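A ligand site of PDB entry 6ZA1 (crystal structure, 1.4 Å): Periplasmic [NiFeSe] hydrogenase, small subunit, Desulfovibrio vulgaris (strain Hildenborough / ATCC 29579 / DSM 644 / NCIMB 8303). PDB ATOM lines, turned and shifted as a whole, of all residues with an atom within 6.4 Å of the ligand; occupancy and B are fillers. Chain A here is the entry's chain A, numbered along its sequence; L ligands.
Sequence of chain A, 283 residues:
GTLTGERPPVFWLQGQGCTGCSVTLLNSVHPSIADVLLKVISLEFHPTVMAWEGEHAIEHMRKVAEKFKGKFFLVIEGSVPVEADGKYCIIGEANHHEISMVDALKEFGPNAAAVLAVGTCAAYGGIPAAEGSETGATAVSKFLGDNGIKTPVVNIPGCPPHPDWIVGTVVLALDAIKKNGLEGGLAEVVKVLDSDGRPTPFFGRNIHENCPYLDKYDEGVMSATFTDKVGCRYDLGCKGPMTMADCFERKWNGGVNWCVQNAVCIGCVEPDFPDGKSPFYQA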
ATOM      1  N   ILE A 207      34.423  10.967  10.622  1.00  0.00           N
ATOM      2  CA  ILE A 207      33.174  10.205  10.585  1.00  0.00           C
ATOM      3  C   ILE A 207      32.020  11.082  10.105  1.00  0.00           C
ATOM      4  O   ILE A 207      31.269  10.724   9.196  1.00  0.00           O
ATOM      5  CB  ILE A 207      32.874   9.586  11.959  1.00  0.00           C
ATOM      6  CG1 ILE A 207      33.889   8.494  12.268  1.00  0.00           C
ATOM      7  CG2 ILE A 207      31.445   9.048  12.008  1.00  0.00           C
ATOM      8  CD1 ILE A 207      33.469   7.500  13.316  1.00  0.00           C
ATOM      9  N   HIS A 208      31.839  12.235  10.754  1.00  0.00           N
ATOM     10  CA  HIS A 208      30.655  13.043  10.532  1.00  0.00           C
ATOM     11  C   HIS A 208      30.595  13.599   9.113  1.00  0.00           C
ATOM     12  O   HIS A 208      29.539  13.594   8.479  1.00  0.00           O
ATOM     13  CB  HIS A 208      30.649  14.136  11.601  1.00  0.00           C
ATOM     14  CG  HIS A 208      29.698  15.261  11.360  1.00  0.00           C
ATOM     15  ND1 HIS A 208      28.362  15.192  11.713  1.00  0.00           N
ATOM     16  CD2 HIS A 208      29.892  16.505  10.863  1.00  0.00           C
ATOM     17  CE1 HIS A 208      27.780  16.337  11.423  1.00  0.00           C
ATOM     18  NE2 HIS A 208      28.676  17.145  10.900  1.00  0.00           N
ATOM     19  N   GLU A 209      31.736  14.059   8.580  1.00  0.00           N
ATOM     20  CA  GLU A 209      31.723  14.636   7.240  1.00  0.00           C
ATOM     21  C   GLU A 209      31.378  13.594   6.176  1.00  0.00           C
ATOM     22  O   GLU A 209      31.012  13.969   5.058  1.00  0.00           O
ATOM     23  CB  GLU A 209      33.070  15.265   6.906  1.00  0.00           C
ATOM     24  CG  GLU A 209      33.437  16.437   7.793  1.00  0.00           C
ATOM     25  CD  GLU A 209      32.424  17.570   7.737  1.00  0.00           C
ATOM     26  OE1 GLU A 209      31.951  17.903   6.631  1.00  0.00           O
ATOM     27  OE2 GLU A 209      32.108  18.132   8.805  1.00  0.00           O
ATOM     28  N   CYS A 211      29.215  10.927   7.023  1.00  0.00           N
ATOM     29  CA  CYS A 211      28.162  10.152   7.668  1.00  0.00           C
ATOM     30  C   CYS A 211      26.912  10.107   6.799  1.00  0.00           C
ATOM     31  O   CYS A 211      26.495  11.139   6.247  1.00  0.00           O
ATOM     32  CB  CYS A 211      27.812  10.764   9.013  1.00  0.00           C
ATOM     33  SG  CYS A 211      26.521   9.836   9.884  1.00  0.00           S
ATOM     34  N   PRO A 212      26.272   8.943   6.682  1.00  0.00           N
ATOM     35  CA  PRO A 212      25.014   8.889   5.904  1.00  0.00           C
ATOM     36  C   PRO A 212      23.900   9.745   6.472  1.00  0.00           C
ATOM     37  O   PRO A 212      22.960  10.065   5.739  1.00  0.00           O
ATOM     38  CB  PRO A 212      24.650   7.390   5.910  1.00  0.00           C
ATOM     39  CG  PRO A 212      25.370   6.829   7.074  1.00  0.00           C
ATOM     40  CD  PRO A 212      26.643   7.622   7.209  1.00  0.00           C
ATOM     41  N   TYR A 213      23.950  10.137   7.746  1.00  0.00           N
ATOM     42  CA  TYR A 213      22.893  10.965   8.320  1.00  0.00           C
ATOM     43  C   TYR A 213      23.226  12.448   8.274  1.00  0.00           C
ATOM     44  O   TYR A 213      22.497  13.253   8.862  1.00  0.00           O
ATOM     45  CB  TYR A 213      22.530  10.477   9.721  1.00  0.00           C
ATOM     46  CG  TYR A 213      22.372   8.964   9.760  1.00  0.00           C
ATOM     47  CD1 TYR A 213      21.285   8.334   9.143  1.00  0.00           C
ATOM     48  CD2 TYR A 213      23.316   8.170  10.387  1.00  0.00           C
ATOM     49  CE1 TYR A 213      21.148   6.949   9.170  1.00  0.00           C
ATOM     50  CE2 TYR A 213      23.192   6.785  10.408  1.00  0.00           C
ATOM     51  CZ  TYR A 213      22.124   6.178   9.802  1.00  0.00           C
ATOM     52  OH  TYR A 213      22.013   4.804   9.840  1.00  0.00           O
ATOM     53  N   LEU A 214      24.285  12.839   7.555  1.00  0.00           N
ATOM     54  CA  LEU A 214      24.676  14.241   7.513  1.00  0.00           C
ATOM     55  C   LEU A 214      23.575  15.135   6.942  1.00  0.00           C
ATOM     56  O   LEU A 214      23.442  16.294   7.354  1.00  0.00           O
ATOM     57  CB  LEU A 214      25.975  14.409   6.724  1.00  0.00           C
ATOM     58  CG  LEU A 214      26.676  15.779   6.765  1.00  0.00           C
ATOM     59  CD1 LEU A 214      27.075  16.179   8.165  1.00  0.00           C
ATOM     60  CD2 LEU A 214      27.896  15.743   5.841  1.00  0.00           C
ATOM     61  N   ASP A 215      22.783  14.622   5.991  1.00  0.00           N
ATOM     62  CA  ASP A 215      21.663  15.409   5.477  1.00  0.00           C
ATOM     63  C   ASP A 215      20.693  15.776   6.592  1.00  0.00           C
ATOM     64  O   ASP A 215      20.214  16.920   6.664  1.00  0.00           O
ATOM     65  CB  ASP A 215      20.959  14.669   4.328  1.00  0.00           C
ATOM     66  CG  ASP A 215      20.328  13.339   4.741  1.00  0.00           C
ATOM     67  OD1 ASP A 215      20.879  12.648   5.612  1.00  0.00           O
ATOM     68  OD2 ASP A 215      19.282  12.986   4.156  1.00  0.00           O
ATOM     69  N   LYS A 216      20.405  14.836   7.503  1.00  0.00           N
ATOM     70  CA  LYS A 216      19.522  15.119   8.619  1.00  0.00           C
ATOM     71  C   LYS A 216      20.141  16.119   9.582  1.00  0.00           C
ATOM     72  O   LYS A 216      19.468  17.021  10.090  1.00  0.00           O
ATOM     73  CB  LYS A 216      19.179  13.822   9.343  1.00  0.00           C
ATOM     74  CG  LYS A 216      18.528  12.760   8.466  1.00  0.00           C
ATOM     75  CD  LYS A 216      17.243  13.281   7.860  1.00  0.00           C
ATOM     76  CE  LYS A 216      16.626  12.258   6.917  1.00  0.00           C
ATOM     77  NZ  LYS A 216      15.526  12.877   6.119  1.00  0.00           N
ATOM     78  N   TYR A 217      21.445  15.970   9.858  1.00  0.00           N
ATOM     79  CA  TYR A 217      22.155  16.950  10.668  1.00  0.00           C
ATOM     80  C   TYR A 217      21.988  18.347  10.087  1.00  0.00           C
ATOM     81  O   TYR A 217      21.614  19.292  10.786  1.00  0.00           O
ATOM     82  CB  TYR A 217      23.629  16.582  10.742  1.00  0.00           C
ATOM     83  CG  TYR A 217      24.492  17.565  11.516  1.00  0.00           C
ATOM     84  CD1 TYR A 217      24.693  17.407  12.885  1.00  0.00           C
ATOM     85  CD2 TYR A 217      25.103  18.633  10.881  1.00  0.00           C
ATOM     86  CE1 TYR A 217      25.480  18.288  13.594  1.00  0.00           C
ATOM     87  CE2 TYR A 217      25.895  19.525  11.584  1.00  0.00           C
ATOM     88  CZ  TYR A 217      26.073  19.350  12.936  1.00  0.00           C
ATOM     89  OH  TYR A 217      26.860  20.231  13.645  1.00  0.00           O
ATOM     90  N   MET A 222      16.706  15.680  14.308  1.00  0.00           N
ATOM     91  CA  MET A 222      17.442  14.929  15.309  1.00  0.00           C
ATOM     92  C   MET A 222      16.542  13.879  15.948  1.00  0.00           C
ATOM     93  O   MET A 222      15.391  14.172  16.300  1.00  0.00           O
ATOM     94  CB  MET A 222      17.923  15.838  16.450  1.00  0.00           C
ATOM     95  CG  MET A 222      18.861  16.926  16.017  1.00  0.00           C
ATOM     96  SD  MET A 222      20.430  16.220  15.510  1.00  0.00           S
ATOM     97  CE  MET A 222      21.207  17.659  14.793  1.00  0.00           C
ATOM     98  N   GLY A 231      16.465  10.173  12.115  1.00  0.00           N
ATOM     99  CA  GLY A 231      17.165  11.399  12.421  1.00  0.00           C
ATOM    100  C   GLY A 231      18.657  11.227  12.649  1.00  0.00           C
ATOM    101  O   GLY A 231      19.186  10.122  12.777  1.00  0.00           O
ATOM    102  N   CYS A 232      19.348  12.371  12.700  1.00  0.00           N
ATOM    103  CA  CYS A 232      20.726  12.425  13.137  1.00  0.00           C
ATOM    104  C   CYS A 232      20.800  12.138  14.634  1.00  0.00           C
ATOM    105  O   CYS A 232      19.859  12.412  15.384  1.00  0.00           O
ATOM    106  CB  CYS A 232      21.329  13.792  12.808  1.00  0.00           C
ATOM    107  SG  CYS A 232      22.878  14.243  13.621  1.00  0.00           S
ATOM    108  N   ARG A 233      21.934  11.575  15.053  1.00  0.00           N
ATOM    109  CA  ARG A 233      22.139  11.105  16.424  1.00  0.00           C
ATOM    110  C   ARG A 233      22.855  12.128  17.308  1.00  0.00           C
ATOM    111  O   ARG A 233      23.191  11.820  18.453  1.00  0.00           O
ATOM    112  CB  ARG A 233      22.942   9.798  16.401  1.00  0.00           C
ATOM    113  CG  ARG A 233      22.208   8.531  15.953  1.00  0.00           C
ATOM    114  CD  ARG A 233      21.822   8.506  14.472  1.00  0.00           C
ATOM    115  NE  ARG A 233      21.648   7.122  14.037  1.00  0.00           N
ATOM    116  CZ  ARG A 233      20.794   6.688  13.110  1.00  0.00           C
ATOM    117  NH1 ARG A 233      19.992   7.533  12.462  1.00  0.00           N
ATOM    118  NH2 ARG A 233      20.752   5.400  12.818  1.00  0.00           N
ATOM    119  N   TYR A 234      23.066  13.349  16.813  1.00  0.00           N
ATOM    120  CA  TYR A 234      23.850  14.326  17.561  1.00  0.00           C
ATOM    121  C   TYR A 234      23.257  14.615  18.938  1.00  0.00           C
ATOM    122  O   TYR A 234      23.991  14.685  19.932  1.00  0.00           O
ATOM    123  CB  TYR A 234      23.924  15.616  16.758  1.00  0.00           C
ATOM    124  CG  TYR A 234      24.748  16.703  17.388  1.00  0.00           C
ATOM    125  CD1 TYR A 234      26.129  16.705  17.288  1.00  0.00           C
ATOM    126  CD2 TYR A 234      24.146  17.737  18.083  1.00  0.00           C
ATOM    127  CE1 TYR A 234      26.879  17.701  17.862  1.00  0.00           C
ATOM    128  CE2 TYR A 234      24.879  18.739  18.654  1.00  0.00           C
ATOM    129  CZ  TYR A 234      26.255  18.718  18.538  1.00  0.00           C
ATOM    130  OH  TYR A 234      26.991  19.730  19.118  1.00  0.00           O
ATOM    131  N   ASP A 235      21.942  14.818  19.013  1.00  0.00           N
ATOM    132  CA  ASP A 235      21.340  15.174  20.298  1.00  0.00           C
ATOM    133  C   ASP A 235      21.399  14.018  21.290  1.00  0.00           C
ATOM    134  O   ASP A 235      21.332  14.242  22.505  1.00  0.00           O
ATOM    135  CB  ASP A 235      19.893  15.617  20.110  1.00  0.00           C
ATOM    136  CG  ASP A 235      19.792  17.057  19.618  1.00  0.00           C
ATOM    137  OD1 ASP A 235      20.827  17.745  19.538  1.00  0.00           O
ATOM    138  OD2 ASP A 235      18.668  17.494  19.323  1.00  0.00           O
ATOM    139  N   CYS A 238      26.099  11.686  19.787  1.00  0.00           N
ATOM    140  CA  CYS A 238      27.067  11.244  18.790  1.00  0.00           C
ATOM    141  C   CYS A 238      28.284  12.153  18.744  1.00  0.00           C
ATOM    142  O   CYS A 238      28.155  13.375  18.631  1.00  0.00           O
ATOM    143  CB  CYS A 238      26.399  11.202  17.420  1.00  0.00           C
ATOM    144  SG  CYS A 238      27.460  10.490  16.159  1.00  0.00           S
ATOM    145  N   LYS A 239      29.464  11.537  18.824  1.00  0.00           N
ATOM    146  CA  LYS A 239      30.739  12.251  18.770  1.00  0.00           C
ATOM    147  C   LYS A 239      31.406  12.148  17.405  1.00  0.00           C
ATOM    148  O   LYS A 239      32.594  12.471  17.272  1.00  0.00           O
ATOM    149  CB  LYS A 239      31.669  11.725  19.871  1.00  0.00           C
ATOM    150  CG  LYS A 239      31.090  11.833  21.283  1.00  0.00           C
ATOM    151  CD  LYS A 239      30.638  13.262  21.594  1.00  0.00           C
ATOM    152  CE  LYS A 239      30.329  13.465  23.076  1.00  0.00           C
ATOM    153  NZ  LYS A 239      29.198  12.615  23.543  1.00  0.00           N
ATOM    154  N   GLY A 240      30.672  11.709  16.380  1.00  0.00           N
ATOM    155  CA  GLY A 240      31.192  11.666  15.034  1.00  0.00           C
ATOM    156  C   GLY A 240      31.869  12.930  14.560  1.00  0.00           C
ATOM    157  O   GLY A 240      32.874  12.853  13.834  1.00  0.00           O
ATOM    158  N   PRO A 241      31.360  14.119  14.916  1.00  0.00           N
ATOM    159  CA  PRO A 241      32.026  15.359  14.468  1.00  0.00           C
ATOM    160  C   PRO A 241      33.482  15.468  14.876  1.00  0.00           C
ATOM    161  O   PRO A 241      34.274  16.103  14.160  1.00  0.00           O
ATOM    162  CB  PRO A 241      31.181  16.466  15.098  1.00  0.00           C
ATOM    163  CG  PRO A 241      29.825  15.863  15.225  1.00  0.00           C
ATOM    164  CD  PRO A 241      30.059  14.397  15.554  1.00  0.00           C
ATOM    165  N   TRP A 258      27.190  -0.707  12.514  1.00  0.00           N
ATOM    166  CA  TRP A 258      28.221   0.161  13.091  1.00  0.00           C
ATOM    167  C   TRP A 258      27.585   1.041  14.152  1.00  0.00           C
ATOM    168  O   TRP A 258      26.362   1.104  14.291  1.00  0.00           O
ATOM    169  CB  TRP A 258      28.975   0.960  12.035  1.00  0.00           C
ATOM    170  CG  TRP A 258      28.212   2.011  11.295  1.00  0.00           C
ATOM    171  CD1 TRP A 258      27.116   1.839  10.512  1.00  0.00           C
ATOM    172  CD2 TRP A 258      28.555   3.403  11.210  1.00  0.00           C
ATOM    173  NE1 TRP A 258      26.725   3.039   9.963  1.00  0.00           N
ATOM    174  CE2 TRP A 258      27.605   4.016  10.368  1.00  0.00           C
ATOM    175  CE3 TRP A 258      29.562   4.191  11.759  1.00  0.00           C
ATOM    176  CZ2 TRP A 258      27.629   5.375  10.082  1.00  0.00           C
ATOM    177  CZ3 TRP A 258      29.594   5.539  11.474  1.00  0.00           C
ATOM    178  CH2 TRP A 258      28.628   6.122  10.642  1.00  0.00           C
ATOM    179  N   VAL A 260      27.107   4.253  14.782  1.00  0.00           N
ATOM    180  CA  VAL A 260      26.179   5.350  14.521  1.00  0.00           C
ATOM    181  C   VAL A 260      24.828   4.817  14.088  1.00  0.00           C
ATOM    182  O   VAL A 260      23.778   5.352  14.485  1.00  0.00           O
ATOM    183  CB  VAL A 260      26.778   6.336  13.496  1.00  0.00           C
ATOM    184  CG1 VAL A 260      25.735   7.350  13.095  1.00  0.00           C
ATOM    185  CG2 VAL A 260      28.004   7.022  14.084  1.00  0.00           C
ATOM    186  N   CYS A 265      28.263   7.179  17.989  1.00  0.00           N
ATOM    187  CA  CYS A 265      29.715   7.094  18.073  1.00  0.00           C
ATOM    188  C   CYS A 265      30.171   7.747  19.370  1.00  0.00           C
ATOM    189  O   CYS A 265      29.673   8.814  19.744  1.00  0.00           O
ATOM    190  CB  CYS A 265      30.348   7.815  16.883  1.00  0.00           C
ATOM    191  SG  CYS A 265      32.148   7.960  16.867  1.00  0.00           S
HETATM  192 FE1  LIG L   1      26.696  11.578  14.285  1.00  0.00          FE
HETATM  193 FE2  LIG L   1      27.312  13.567  12.478  1.00  0.00          FE
HETATM  194 FE3  LIG L   1      24.718  13.073  13.008  1.00  0.00          FE
HETATM  195 FE4  LIG L   1      26.259  11.284  11.592  1.00  0.00          FE
HETATM  196  S1  LIG L   1      25.617  13.381  10.922  1.00  0.00           S
HETATM  197  S2  LIG L   1      24.753  10.803  13.282  1.00  0.00           S
HETATM  198  S3  LIG L   1      28.298  11.510  12.646  1.00  0.00           S
HETATM  199  S4  LIG L   1      26.296  13.802  14.531  1.00  0.00           S
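N of His 208 is in hydrogen-bond range of O of Gly 240 (3.3 Å). SG of Cys 232 lies close to N of Tyr 234. SG of Cys 232 sits close to SD of Met 222. The backbone NH (N) of Cys 238 sits at hydrogen-bond distance from the backbone carbonyl oxygen (O) of Arg 233, 3.2 Å away. The side-chain sulfur of Cys 238 lies close to the backbone NH of Gly 240 (3.4 Å). NE of Arg 233 sits at hydrogen-bond distance from O of Val 260. NH2 of Arg 233 lies within hydrogen-bond range of OH of Tyr 213 (3.3 Å). NH1 of Arg 233 sits at hydrogen-bond distance from O of Gly 231, 2.7 Å away.
S1 of the ligand sits close to O of Tyr 213 (3.7 Å). Tyr 217 touches the ligand. Tyr 234 touches the ligand. Gly 240 touches the ligand. CD of Pro 241 touches S4 of the ligand (3.9 Å). Val 260 touches the ligand. Hydrophobic or aromatic side chains that line the ligand: His 208, Tyr 217, Tyr 234, Pro 241 and Val 260. The nearest printed residue that does not touch the ligand is Ile 207 (4.05 Å).
An iron atom (FE2) of the ligand is bound by a ring nitrogen (ND1) of His 208. The side-chain sulfur (SG) of Cys 211 binds an iron atom (FE4) of the ligand (2.3 Å). The side-chain sulfur (SG) of Cys 232 is bound to an iron atom (FE3) of the ligand (2.3 Å). The side-chain sulfur (SG) of Cys 238 binds an iron atom (FE1) of the ligand (2.3 Å). The backbone NH of Arg 233 sits close to a sulfur (S2) of the ligand. The backbone NH (N) of Leu 214 sits close to a sulfur (S1) of the ligand, at 3.7 Å.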
